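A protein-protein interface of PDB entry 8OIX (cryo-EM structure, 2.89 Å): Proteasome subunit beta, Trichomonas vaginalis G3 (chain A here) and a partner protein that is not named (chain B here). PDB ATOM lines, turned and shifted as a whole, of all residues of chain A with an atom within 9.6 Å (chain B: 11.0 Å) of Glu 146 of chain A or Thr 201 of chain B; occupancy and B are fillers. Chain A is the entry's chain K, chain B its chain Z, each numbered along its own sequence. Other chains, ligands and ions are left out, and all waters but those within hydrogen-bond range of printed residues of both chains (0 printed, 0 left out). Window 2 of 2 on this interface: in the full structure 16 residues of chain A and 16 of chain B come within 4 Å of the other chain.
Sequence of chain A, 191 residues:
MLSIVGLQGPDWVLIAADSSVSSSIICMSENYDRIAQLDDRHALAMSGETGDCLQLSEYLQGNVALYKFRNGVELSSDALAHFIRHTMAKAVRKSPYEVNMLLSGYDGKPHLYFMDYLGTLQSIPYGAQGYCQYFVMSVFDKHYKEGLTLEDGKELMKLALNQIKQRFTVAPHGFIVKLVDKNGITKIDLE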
ATOM      1  N   LEU A   7     -15.277  21.385 -31.303  1.00  0.00           N
ATOM      2  CA  LEU A   7     -15.315  19.959 -30.993  1.00  0.00           C
ATOM      3  C   LEU A   7     -15.595  19.201 -32.283  1.00  0.00           C
ATOM      4  O   LEU A   7     -16.688  19.311 -32.839  1.00  0.00           O
ATOM      5  CB  LEU A   7     -16.383  19.657 -29.942  1.00  0.00           C
ATOM      6  CG  LEU A   7     -16.614  18.195 -29.576  1.00  0.00           C
ATOM      7  CD1 LEU A   7     -15.354  17.623 -28.975  1.00  0.00           C
ATOM      8  CD2 LEU A   7     -17.775  18.065 -28.613  1.00  0.00           C
ATOM      9  N   GLN A   8     -14.623  18.426 -32.751  1.00  0.00           N
ATOM     10  CA  GLN A   8     -14.763  17.689 -33.999  1.00  0.00           C
ATOM     11  C   GLN A   8     -15.290  16.288 -33.725  1.00  0.00           C
ATOM     12  O   GLN A   8     -14.792  15.593 -32.833  1.00  0.00           O
ATOM     13  CB  GLN A   8     -13.424  17.612 -34.733  1.00  0.00           C
ATOM     14  CG  GLN A   8     -13.510  17.019 -36.123  1.00  0.00           C
ATOM     15  CD  GLN A   8     -12.144  16.778 -36.727  1.00  0.00           C
ATOM     16  OE1 GLN A   8     -11.933  15.798 -37.440  1.00  0.00           O
ATOM     17  NE2 GLN A   8     -11.205  17.671 -36.440  1.00  0.00           N
ATOM     18  N   GLY A   9     -16.297  15.879 -34.490  1.00  0.00           N
ATOM     19  CA  GLY A   9     -16.847  14.552 -34.384  1.00  0.00           C
ATOM     20  C   GLY A   9     -16.539  13.721 -35.611  1.00  0.00           C
ATOM     21  O   GLY A   9     -15.815  14.152 -36.512  1.00  0.00           O
ATOM     22  N   PRO A  10     -17.063  12.494 -35.657  1.00  0.00           N
ATOM     23  CA  PRO A  10     -16.810  11.635 -36.826  1.00  0.00           C
ATOM     24  C   PRO A  10     -17.296  12.226 -38.138  1.00  0.00           C
ATOM     25  O   PRO A  10     -16.634  12.054 -39.168  1.00  0.00           O
ATOM     26  CB  PRO A  10     -17.553  10.338 -36.473  1.00  0.00           C
ATOM     27  CG  PRO A  10     -18.543  10.727 -35.430  1.00  0.00           C
ATOM     28  CD  PRO A  10     -17.908  11.832 -34.653  1.00  0.00           C
ATOM     29  N   ASP A  11     -18.452  12.897 -38.139  1.00  0.00           N
ATOM     30  CA  ASP A  11     -18.978  13.494 -39.360  1.00  0.00           C
ATOM     31  C   ASP A  11     -19.624  14.851 -39.095  1.00  0.00           C
ATOM     32  O   ASP A  11     -20.565  15.239 -39.793  1.00  0.00           O
ATOM     33  CB  ASP A  11     -19.979  12.559 -40.041  1.00  0.00           C
ATOM     34  CG  ASP A  11     -20.930  11.905 -39.060  1.00  0.00           C
ATOM     35  OD1 ASP A  11     -20.967  12.333 -37.888  1.00  0.00           O
ATOM     36  OD2 ASP A  11     -21.638  10.957 -39.459  1.00  0.00           O
ATOM     37  N   TRP A  12     -19.132  15.581 -38.098  1.00  0.00           N
ATOM     38  CA  TRP A  12     -19.695  16.877 -37.746  1.00  0.00           C
ATOM     39  C   TRP A  12     -18.668  17.644 -36.930  1.00  0.00           C
ATOM     40  O   TRP A  12     -17.691  17.076 -36.436  1.00  0.00           O
ATOM     41  CB  TRP A  12     -21.001  16.718 -36.963  1.00  0.00           C
ATOM     42  CG  TRP A  12     -20.884  15.771 -35.805  1.00  0.00           C
ATOM     43  CD1 TRP A  12     -21.297  14.473 -35.766  1.00  0.00           C
ATOM     44  CD2 TRP A  12     -20.311  16.047 -34.521  1.00  0.00           C
ATOM     45  NE1 TRP A  12     -21.016  13.922 -34.541  1.00  0.00           N
ATOM     46  CE2 TRP A  12     -20.411  14.869 -33.758  1.00  0.00           C
ATOM     47  CE3 TRP A  12     -19.725  17.176 -33.942  1.00  0.00           C
ATOM     48  CZ2 TRP A  12     -19.947  14.788 -32.449  1.00  0.00           C
ATOM     49  CZ3 TRP A  12     -19.265  17.092 -32.645  1.00  0.00           C
ATOM     50  CH2 TRP A  12     -19.376  15.908 -31.913  1.00  0.00           C
ATOM     51  N   GLN A 122      -3.292  23.983 -36.757  1.00  0.00           N
ATOM     52  CA  GLN A 122      -3.253  22.602 -36.291  1.00  0.00           C
ATOM     53  C   GLN A 122      -4.651  22.013 -36.335  1.00  0.00           C
ATOM     54  O   GLN A 122      -5.558  22.525 -35.674  1.00  0.00           O
ATOM     55  CB  GLN A 122      -2.689  22.518 -34.877  1.00  0.00           C
ATOM     56  CG  GLN A 122      -2.669  21.121 -34.292  1.00  0.00           C
ATOM     57  CD  GLN A 122      -1.906  20.138 -35.152  1.00  0.00           C
ATOM     58  OE1 GLN A 122      -0.850  20.460 -35.694  1.00  0.00           O
ATOM     59  NE2 GLN A 122      -2.436  18.929 -35.281  1.00  0.00           N
ATOM     60  N   SER A 123      -4.825  20.946 -37.112  1.00  0.00           N
ATOM     61  CA  SER A 123      -6.067  20.189 -37.060  1.00  0.00           C
ATOM     62  C   SER A 123      -6.204  19.533 -35.693  1.00  0.00           C
ATOM     63  O   SER A 123      -5.281  18.863 -35.219  1.00  0.00           O
ATOM     64  CB  SER A 123      -6.096  19.135 -38.163  1.00  0.00           C
ATOM     65  OG  SER A 123      -7.306  18.398 -38.125  1.00  0.00           O
ATOM     66  N   ILE A 124      -7.354  19.724 -35.058  1.00  0.00           N
ATOM     67  CA  ILE A 124      -7.567  19.232 -33.699  1.00  0.00           C
ATOM     68  C   ILE A 124      -8.893  18.486 -33.610  1.00  0.00           C
ATOM     69  O   ILE A 124      -9.860  18.859 -34.288  1.00  0.00           O
ATOM     70  CB  ILE A 124      -7.526  20.390 -32.690  1.00  0.00           C
ATOM     71  CG1 ILE A 124      -8.304  21.584 -33.241  1.00  0.00           C
ATOM     72  CG2 ILE A 124      -6.091  20.778 -32.381  1.00  0.00           C
ATOM     73  CD1 ILE A 124      -8.660  22.615 -32.210  1.00  0.00           C
ATOM     74  N   PRO A 125      -8.983  17.426 -32.801  1.00  0.00           N
ATOM     75  CA  PRO A 125     -10.304  16.851 -32.516  1.00  0.00           C
ATOM     76  C   PRO A 125     -11.168  17.778 -31.689  1.00  0.00           C
ATOM     77  O   PRO A 125     -12.397  17.757 -31.817  1.00  0.00           O
ATOM     78  CB  PRO A 125      -9.966  15.561 -31.759  1.00  0.00           C
ATOM     79  CG  PRO A 125      -8.666  15.864 -31.097  1.00  0.00           C
ATOM     80  CD  PRO A 125      -7.911  16.747 -32.055  1.00  0.00           C
ATOM     81  N   TYR A 126     -10.553  18.578 -30.826  1.00  0.00           N
ATOM     82  CA  TYR A 126     -11.250  19.571 -30.028  1.00  0.00           C
ATOM     83  C   TYR A 126     -10.229  20.599 -29.574  1.00  0.00           C
ATOM     84  O   TYR A 126      -9.026  20.328 -29.532  1.00  0.00           O
ATOM     85  CB  TYR A 126     -11.969  18.936 -28.835  1.00  0.00           C
ATOM     86  CG  TYR A 126     -11.162  17.875 -28.128  1.00  0.00           C
ATOM     87  CD1 TYR A 126     -10.094  18.215 -27.312  1.00  0.00           C
ATOM     88  CD2 TYR A 126     -11.474  16.532 -28.269  1.00  0.00           C
ATOM     89  CE1 TYR A 126      -9.358  17.251 -26.665  1.00  0.00           C
ATOM     90  CE2 TYR A 126     -10.744  15.560 -27.625  1.00  0.00           C
ATOM     91  CZ  TYR A 126      -9.688  15.924 -26.823  1.00  0.00           C
ATOM     92  OH  TYR A 126      -8.955  14.958 -26.178  1.00  0.00           O
ATOM     93  N   PHE A 140     -12.908  17.732 -22.414  1.00  0.00           N
ATOM     94  CA  PHE A 140     -12.865  16.971 -23.653  1.00  0.00           C
ATOM     95  C   PHE A 140     -12.019  15.726 -23.461  1.00  0.00           C
ATOM     96  O   PHE A 140     -12.479  14.603 -23.700  1.00  0.00           O
ATOM     97  CB  PHE A 140     -12.315  17.834 -24.783  1.00  0.00           C
ATOM     98  CG  PHE A 140     -13.253  18.909 -25.237  1.00  0.00           C
ATOM     99  CD1 PHE A 140     -14.612  18.670 -25.314  1.00  0.00           C
ATOM    100  CD2 PHE A 140     -12.776  20.156 -25.592  1.00  0.00           C
ATOM    101  CE1 PHE A 140     -15.478  19.654 -25.733  1.00  0.00           C
ATOM    102  CE2 PHE A 140     -13.636  21.143 -26.013  1.00  0.00           C
ATOM    103  CZ  PHE A 140     -14.991  20.892 -26.082  1.00  0.00           C
ATOM    104  N   ASP A 141     -10.810  15.907 -22.924  1.00  0.00           N
ATOM    105  CA  ASP A 141      -9.937  14.770 -22.672  1.00  0.00           C
ATOM    106  C   ASP A 141     -10.635  13.755 -21.786  1.00  0.00           C
ATOM    107  O   ASP A 141     -10.469  12.543 -21.962  1.00  0.00           O
ATOM    108  CB  ASP A 141      -8.633  15.241 -22.028  1.00  0.00           C
ATOM    109  CG  ASP A 141      -7.855  16.188 -22.913  1.00  0.00           C
ATOM    110  OD1 ASP A 141      -8.087  16.183 -24.137  1.00  0.00           O
ATOM    111  OD2 ASP A 141      -7.009  16.937 -22.383  1.00  0.00           O
ATOM    112  N   HIS A 143     -13.937  13.256 -21.477  1.00  0.00           N
ATOM    113  CA  HIS A 143     -15.220  12.747 -21.941  1.00  0.00           C
ATOM    114  C   HIS A 143     -15.325  12.518 -23.442  1.00  0.00           C
ATOM    115  O   HIS A 143     -16.373  12.047 -23.899  1.00  0.00           O
ATOM    116  CB  HIS A 143     -16.347  13.684 -21.494  1.00  0.00           C
ATOM    117  CG  HIS A 143     -16.504  13.762 -20.010  1.00  0.00           C
ATOM    118  ND1 HIS A 143     -17.369  12.949 -19.310  1.00  0.00           N
ATOM    119  CD2 HIS A 143     -15.901  14.549 -19.088  1.00  0.00           C
ATOM    120  CE1 HIS A 143     -17.295  13.233 -18.023  1.00  0.00           C
ATOM    121  NE2 HIS A 143     -16.408  14.197 -17.860  1.00  0.00           N
ATOM    122  N   TYR A 144     -14.297  12.826 -24.225  1.00  0.00           N
ATOM    123  CA  TYR A 144     -14.391  12.613 -25.661  1.00  0.00           C
ATOM    124  C   TYR A 144     -14.066  11.165 -25.999  1.00  0.00           C
ATOM    125  O   TYR A 144     -13.044  10.628 -25.562  1.00  0.00           O
ATOM    126  CB  TYR A 144     -13.458  13.552 -26.421  1.00  0.00           C
ATOM    127  CG  TYR A 144     -13.651  13.505 -27.918  1.00  0.00           C
ATOM    128  CD1 TYR A 144     -12.927  12.624 -28.709  1.00  0.00           C
ATOM    129  CD2 TYR A 144     -14.576  14.327 -28.540  1.00  0.00           C
ATOM    130  CE1 TYR A 144     -13.111  12.577 -30.076  1.00  0.00           C
ATOM    131  CE2 TYR A 144     -14.764  14.287 -29.907  1.00  0.00           C
ATOM    132  CZ  TYR A 144     -14.028  13.412 -30.670  1.00  0.00           C
ATOM    133  OH  TYR A 144     -14.215  13.368 -32.031  1.00  0.00           O
ATOM    134  N   LYS A 145     -14.942  10.539 -26.777  1.00  0.00           N
ATOM    135  CA  LYS A 145     -14.736   9.191 -27.282  1.00  0.00           C
ATOM    136  C   LYS A 145     -14.782   9.227 -28.801  1.00  0.00           C
ATOM    137  O   LYS A 145     -15.626   9.911 -29.386  1.00  0.00           O
ATOM    138  CB  LYS A 145     -15.798   8.226 -26.745  1.00  0.00           C
ATOM    139  CG  LYS A 145     -16.042   8.335 -25.249  1.00  0.00           C
ATOM    140  CD  LYS A 145     -14.873   7.788 -24.448  1.00  0.00           C
ATOM    141  CE  LYS A 145     -14.755   8.486 -23.101  1.00  0.00           C
ATOM    142  NZ  LYS A 145     -16.029   8.442 -22.330  1.00  0.00           N
ATOM    143  N   GLU A 146     -13.862   8.506 -29.437  1.00  0.00           N
ATOM    144  CA  GLU A 146     -13.861   8.429 -30.891  1.00  0.00           C
ATOM    145  C   GLU A 146     -15.156   7.791 -31.379  1.00  0.00           C
ATOM    146  O   GLU A 146     -15.654   6.827 -30.793  1.00  0.00           O
ATOM    147  CB  GLU A 146     -12.654   7.630 -31.385  1.00  0.00           C
ATOM    148  CG  GLU A 146     -11.307   8.311 -31.164  1.00  0.00           C
ATOM    149  CD  GLU A 146     -10.831   8.240 -29.723  1.00  0.00           C
ATOM    150  OE1 GLU A 146     -11.496   7.572 -28.903  1.00  0.00           O
ATOM    151  OE2 GLU A 146      -9.788   8.855 -29.410  1.00  0.00           O
ATOM    152  N   GLY A 147     -15.702   8.337 -32.463  1.00  0.00           N
ATOM    153  CA  GLY A 147     -17.016   7.923 -32.909  1.00  0.00           C
ATOM    154  C   GLY A 147     -18.153   8.529 -32.123  1.00  0.00           C
ATOM    155  O   GLY A 147     -19.264   7.991 -32.146  1.00  0.00           O
ATOM    156  N   LEU A 148     -17.899   9.626 -31.412  1.00  0.00           N
ATOM    157  CA  LEU A 148     -18.919  10.293 -30.613  1.00  0.00           C
ATOM    158  C   LEU A 148     -20.135  10.639 -31.461  1.00  0.00           C
ATOM    159  O   LEU A 148     -20.008  11.196 -32.552  1.00  0.00           O
ATOM    160  CB  LEU A 148     -18.324  11.561 -29.996  1.00  0.00           C
ATOM    161  CG  LEU A 148     -18.963  12.166 -28.749  1.00  0.00           C
ATOM    162  CD1 LEU A 148     -18.760  11.250 -27.555  1.00  0.00           C
ATOM    163  CD2 LEU A 148     -18.367  13.534 -28.476  1.00  0.00           C
ATOM    164  N   THR A 149     -21.318  10.310 -30.956  1.00  0.00           N
ATOM    165  CA  THR A 149     -22.533  10.669 -31.669  1.00  0.00           C
ATOM    166  C   THR A 149     -22.764  12.175 -31.596  1.00  0.00           C
ATOM    167  O   THR A 149     -22.211  12.876 -30.745  1.00  0.00           O
ATOM    168  CB  THR A 149     -23.741   9.920 -31.109  1.00  0.00           C
ATOM    169  OG1 THR A 149     -23.752  10.023 -29.682  1.00  0.00           O
ATOM    170  CG2 THR A 149     -23.689   8.453 -31.505  1.00  0.00           C
ATOM    171  N   ASP A 152     -24.212  12.959 -28.251  1.00  0.00           N
ATOM    172  CA  ASP A 152     -23.120  12.953 -27.283  1.00  0.00           C
ATOM    173  C   ASP A 152     -22.184  14.131 -27.509  1.00  0.00           C
ATOM    174  O   ASP A 152     -21.639  14.693 -26.552  1.00  0.00           O
ATOM    175  CB  ASP A 152     -22.350  11.635 -27.356  1.00  0.00           C
ATOM    176  CG  ASP A 152     -23.111  10.482 -26.740  1.00  0.00           C
ATOM    177  OD1 ASP A 152     -24.299  10.665 -26.397  1.00  0.00           O
ATOM    178  OD2 ASP A 152     -22.522   9.390 -26.594  1.00  0.00           O
ATOM    179  N   LEU A 156     -21.277  16.935 -24.786  1.00  0.00           N
ATOM    180  CA  LEU A 156     -19.907  17.265 -24.402  1.00  0.00           C
ATOM    181  C   LEU A 156     -19.614  18.750 -24.583  1.00  0.00           C
ATOM    182  O   LEU A 156     -18.961  19.368 -23.732  1.00  0.00           O
ATOM    183  CB  LEU A 156     -18.927  16.417 -25.212  1.00  0.00           C
ATOM    184  CG  LEU A 156     -17.440  16.645 -24.952  1.00  0.00           C
ATOM    185  CD1 LEU A 156     -17.131  16.546 -23.472  1.00  0.00           C
ATOM    186  CD2 LEU A 156     -16.608  15.649 -25.740  1.00  0.00           C
ATOM    187  N   TYR B 161      -4.247  14.079 -13.632  1.00  0.00           N
ATOM    188  CA  TYR B 161      -3.637  13.578 -14.859  1.00  0.00           C
ATOM    189  C   TYR B 161      -3.978  14.462 -16.051  1.00  0.00           C
ATOM    190  O   TYR B 161      -3.107  14.774 -16.871  1.00  0.00           O
ATOM    191  CB  TYR B 161      -4.084  12.140 -15.121  1.00  0.00           C
ATOM    192  CG  TYR B 161      -4.123  11.782 -16.588  1.00  0.00           C
ATOM    193  CD1 TYR B 161      -2.952  11.663 -17.325  1.00  0.00           C
ATOM    194  CD2 TYR B 161      -5.329  11.576 -17.238  1.00  0.00           C
ATOM    195  CE1 TYR B 161      -2.984  11.346 -18.665  1.00  0.00           C
ATOM    196  CE2 TYR B 161      -5.371  11.256 -18.578  1.00  0.00           C
ATOM    197  CZ  TYR B 161      -4.195  11.142 -19.287  1.00  0.00           C
ATOM    198  OH  TYR B 161      -4.232  10.823 -20.624  1.00  0.00           O
ATOM    199  N   TYR B 165      -1.469  16.652 -18.349  1.00  0.00           N
ATOM    200  CA  TYR B 165      -1.447  16.555 -19.802  1.00  0.00           C
ATOM    201  C   TYR B 165      -1.593  17.927 -20.446  1.00  0.00           C
ATOM    202  O   TYR B 165      -0.820  18.290 -21.340  1.00  0.00           O
ATOM    203  CB  TYR B 165      -2.547  15.609 -20.285  1.00  0.00           C
ATOM    204  CG  TYR B 165      -2.599  15.479 -21.788  1.00  0.00           C
ATOM    205  CD1 TYR B 165      -3.326  16.379 -22.556  1.00  0.00           C
ATOM    206  CD2 TYR B 165      -1.900  14.477 -22.444  1.00  0.00           C
ATOM    207  CE1 TYR B 165      -3.368  16.277 -23.922  1.00  0.00           C
ATOM    208  CE2 TYR B 165      -1.938  14.367 -23.816  1.00  0.00           C
ATOM    209  CZ  TYR B 165      -2.674  15.271 -24.548  1.00  0.00           C
ATOM    210  OH  TYR B 165      -2.722  15.179 -25.915  1.00  0.00           O
ATOM    211  N   ARG B 166      -2.582  18.703 -20.012  1.00  0.00           N
ATOM    212  CA  ARG B 166      -2.867  19.969 -20.671  1.00  0.00           C
ATOM    213  C   ARG B 166      -2.025  21.131 -20.160  1.00  0.00           C
ATOM    214  O   ARG B 166      -2.016  22.188 -20.798  1.00  0.00           O
ATOM    215  CB  ARG B 166      -4.349  20.312 -20.525  1.00  0.00           C
ATOM    216  CG  ARG B 166      -5.247  19.447 -21.379  1.00  0.00           C
ATOM    217  CD  ARG B 166      -4.989  19.696 -22.851  1.00  0.00           C
ATOM    218  NE  ARG B 166      -5.685  18.735 -23.697  1.00  0.00           N
ATOM    219  CZ  ARG B 166      -5.530  18.647 -25.010  1.00  0.00           C
ATOM    220  NH1 ARG B 166      -4.713  19.455 -25.664  1.00  0.00           N
ATOM    221  NH2 ARG B 166      -6.212  17.726 -25.683  1.00  0.00           N
ATOM    222  N   HIS B 196      -2.053   7.809 -18.660  1.00  0.00           N
ATOM    223  CA  HIS B 196      -2.396   8.176 -20.026  1.00  0.00           C
ATOM    224  C   HIS B 196      -2.804   6.946 -20.824  1.00  0.00           C
ATOM    225  O   HIS B 196      -2.128   5.914 -20.787  1.00  0.00           O
ATOM    226  CB  HIS B 196      -1.217   8.879 -20.698  1.00  0.00           C
ATOM    227  CG  HIS B 196      -1.540   9.441 -22.046  1.00  0.00           C
ATOM    228  ND1 HIS B 196      -2.052  10.709 -22.219  1.00  0.00           N
ATOM    229  CD2 HIS B 196      -1.434   8.907 -23.285  1.00  0.00           C
ATOM    230  CE1 HIS B 196      -2.242  10.933 -23.506  1.00  0.00           C
ATOM    231  NE2 HIS B 196      -1.874   9.855 -24.175  1.00  0.00           N
ATOM    232  N   ASP B 197      -3.913   7.060 -21.547  1.00  0.00           N
ATOM    233  CA  ASP B 197      -4.417   5.981 -22.389  1.00  0.00           C
ATOM    234  C   ASP B 197      -3.903   6.224 -23.801  1.00  0.00           C
ATOM    235  O   ASP B 197      -4.382   7.124 -24.498  1.00  0.00           O
ATOM    236  CB  ASP B 197      -5.943   5.928 -22.351  1.00  0.00           C
ATOM    237  CG  ASP B 197      -6.501   4.634 -22.917  1.00  0.00           C
ATOM    238  OD1 ASP B 197      -5.873   4.049 -23.824  1.00  0.00           O
ATOM    239  OD2 ASP B 197      -7.573   4.199 -22.450  1.00  0.00           O
ATOM    240  N   PHE B 198      -2.930   5.422 -24.220  1.00  0.00           N
ATOM    241  CA  PHE B 198      -2.309   5.580 -25.527  1.00  0.00           C
ATOM    242  C   PHE B 198      -3.069   4.865 -26.634  1.00  0.00           C
ATOM    243  O   PHE B 198      -2.659   4.944 -27.796  1.00  0.00           O
ATOM    244  CB  PHE B 198      -0.860   5.095 -25.477  1.00  0.00           C
ATOM    245  CG  PHE B 198       0.023   5.947 -24.617  1.00  0.00           C
ATOM    246  CD1 PHE B 198       0.125   5.712 -23.258  1.00  0.00           C
ATOM    247  CD2 PHE B 198       0.728   7.002 -25.164  1.00  0.00           C
ATOM    248  CE1 PHE B 198       0.927   6.505 -22.465  1.00  0.00           C
ATOM    249  CE2 PHE B 198       1.530   7.798 -24.375  1.00  0.00           C
ATOM    250  CZ  PHE B 198       1.631   7.548 -23.025  1.00  0.00           C
ATOM    251  N   SER B 199      -4.158   4.173 -26.306  1.00  0.00           N
ATOM    252  CA  SER B 199      -5.050   3.662 -27.335  1.00  0.00           C
ATOM    253  C   SER B 199      -5.917   4.760 -27.932  1.00  0.00           C
ATOM    254  O   SER B 199      -6.416   4.600 -29.050  1.00  0.00           O
ATOM    255  CB  SER B 199      -5.934   2.551 -26.765  1.00  0.00           C
ATOM    256  OG  SER B 199      -5.148   1.492 -26.248  1.00  0.00           O
ATOM    257  N   LYS B 200      -6.105   5.861 -27.210  1.00  0.00           N
ATOM    258  CA  LYS B 200      -6.837   7.000 -27.743  1.00  0.00           C
ATOM    259  C   LYS B 200      -5.972   7.756 -28.743  1.00  0.00           C
ATOM    260  O   LYS B 200      -4.763   7.910 -28.553  1.00  0.00           O
ATOM    261  CB  LYS B 200      -7.275   7.933 -26.613  1.00  0.00           C
ATOM    262  CG  LYS B 200      -8.622   7.596 -25.972  1.00  0.00           C
ATOM    263  CD  LYS B 200      -8.711   6.145 -25.520  1.00  0.00           C
ATOM    264  CE  LYS B 200     -10.082   5.821 -24.955  1.00  0.00           C
ATOM    265  NZ  LYS B 200     -10.193   4.388 -24.568  1.00  0.00           N
ATOM    266  N   THR B 201      -6.599   8.230 -29.817  1.00  0.00           N
ATOM    267  CA  THR B 201      -5.906   8.994 -30.843  1.00  0.00           C
ATOM    268  C   THR B 201      -6.186  10.488 -30.763  1.00  0.00           C
ATOM    269  O   THR B 201      -5.643  11.249 -31.569  1.00  0.00           O
ATOM    270  CB  THR B 201      -6.286   8.477 -32.235  1.00  0.00           C
ATOM    271  OG1 THR B 201      -7.702   8.597 -32.423  1.00  0.00           O
ATOM    272  CG2 THR B 201      -5.882   7.018 -32.386  1.00  0.00           C
ATOM    273  N   THR B 202      -7.018  10.927 -29.818  1.00  0.00           N
ATOM    274  CA  THR B 202      -7.343  12.341 -29.695  1.00  0.00           C
ATOM    275  C   THR B 202      -6.434  13.086 -28.730  1.00  0.00           C
ATOM    276  O   THR B 202      -6.278  14.304 -28.868  1.00  0.00           O
ATOM    277  CB  THR B 202      -8.797  12.514 -29.249  1.00  0.00           C
ATOM    278  OG1 THR B 202      -9.035  11.733 -28.072  1.00  0.00           O
ATOM    279  CG2 THR B 202      -9.734  12.058 -30.348  1.00  0.00           C
ATOM    280  N   PHE B 203      -5.826  12.388 -27.776  1.00  0.00           N
ATOM    281  CA  PHE B 203      -4.918  13.015 -26.822  1.00  0.00           C
ATOM    282  C   PHE B 203      -4.161  11.953 -26.033  1.00  0.00           C
ATOM    283  O   PHE B 203      -3.224  11.340 -26.543  1.00  0.00           O
ATOM    284  CB  PHE B 203      -5.682  13.939 -25.868  1.00  0.00           C
ATOM    285  CG  PHE B 203      -6.216  13.248 -24.648  1.00  0.00           C
ATOM    286  CD1 PHE B 203      -7.363  12.479 -24.719  1.00  0.00           C
ATOM    287  CD2 PHE B 203      -5.579  13.382 -23.428  1.00  0.00           C
ATOM    288  CE1 PHE B 203      -7.856  11.846 -23.597  1.00  0.00           C
ATOM    289  CE2 PHE B 203      -6.066  12.753 -22.304  1.00  0.00           C
ATOM    290  CZ  PHE B 203      -7.207  11.984 -22.388  1.00  0.00           C
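Hydrophobic or aromatic side chains of chain A within 4 Å of the printed part of chain B: Pro 125, Tyr 126 and Tyr 144.
Along chain B the printed residues that touch a printed residue of chain A span positions 165 to 203.
Printed residues of chain B within 4 Å of Tyr 126 of chain A: Arg 166 (3.3 Å), Thr 202 (3.7 Å) and Phe 203 (3.3 Å).
Glu 146 of chain A touches just these residues of chain B: Lys 200 (3.8 Å), Thr 201 (3.3 Å) and Thr 202 (3.3 Å).
No residue of chain B comes within 4 Å of Gly 147 of chain A.
No residue of chain B comes within 4 Å of Leu 148 of chain A.
Thr 149 of chain A touches none of the printed residues of chain B.
Of the printed residues of chain A, Tyr 165 of chain B touches Asp 141.
Of the printed residues of chain A, Arg 166 of chain B touches Tyr 126 and Asp 141.
Of the printed residues of chain A, Thr 201 of chain B touches Glu 146 (3.3 Å).
Thr 202 of chain B touches just these residues of chain A: Pro 125 (3.6 Å), Tyr 126 (3.7 Å), Tyr 144 (3.4 Å) and Glu 146 (3.3 Å).
Of the printed residues of chain A, Phe 203 of chain B touches Tyr 126 (3.3 Å) and Asp 141 (3.2 Å).
NE of Arg 166 of chain B lies within salt-bridge range of OD2 of Asp 141 of chain A.
The side-chain carboxylate (OE2) of Glu 146 of chain A lies within hydrogen-bond range of the backbone NH (N) of Thr 201 of chain B, at 3.3 Å.
The side-chain hydroxyl (OG1) of Thr 202 of chain B is in hydrogen-bond range of the side-chain carboxylate (OE2) of Glu 146 of chain A (3.3 Å).
The backbone NH of Gln 8 of chain A lies within hydrogen-bond range of the backbone carbonyl oxygen of Pro 125 of chain A (2.5 Å).
OH of Tyr 144 of chain A sits at hydrogen-bond distance from O of Gln 8 of chain A (2.4 Å).
The side-chain hydroxyl of Tyr 126 of chain A sits at hydrogen-bond distance from the side-chain carboxylate of Asp 141 of chain A, at 2.5 Å.
The backbone carbonyl oxygen of Phe 203 of chain B sits at hydrogen-bond distance from a ring nitrogen (NE2) of His 196 of chain B.
The side-chain carboxylate (OD2) of Asp 197 of chain B lies within salt-bridge range of the side-chain amino group (NZ) of Lys 200 of chain B (3.4 Å).
CG of Pro 125 of chain A touches O of Thr 202 of chain B (3.6 Å).
CE1 of Tyr 126 of chain A touches NH2 of Arg 166 of chain B, at 3.3 Å.
OH of Tyr 126 of chain A touches OG1 of Thr 202 of chain B (3.7 Å).
CD1 of Phe 203 of chain B touches OH of Tyr 126 of chain A, at 3.3 Å.
OD2 of Asp 141 of chain A touches CD1 of Tyr 165 of chain B, 3.7 Å away.
Phe 203 of chain B touches Asp 141 of chain A (CE1 to O, 3.2 Å).
CG2 of Thr 202 of chain B touches CE1 of Tyr 144 of chain A (3.4 Å).
Glu 146 of chain A touches Lys 200 of chain B.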
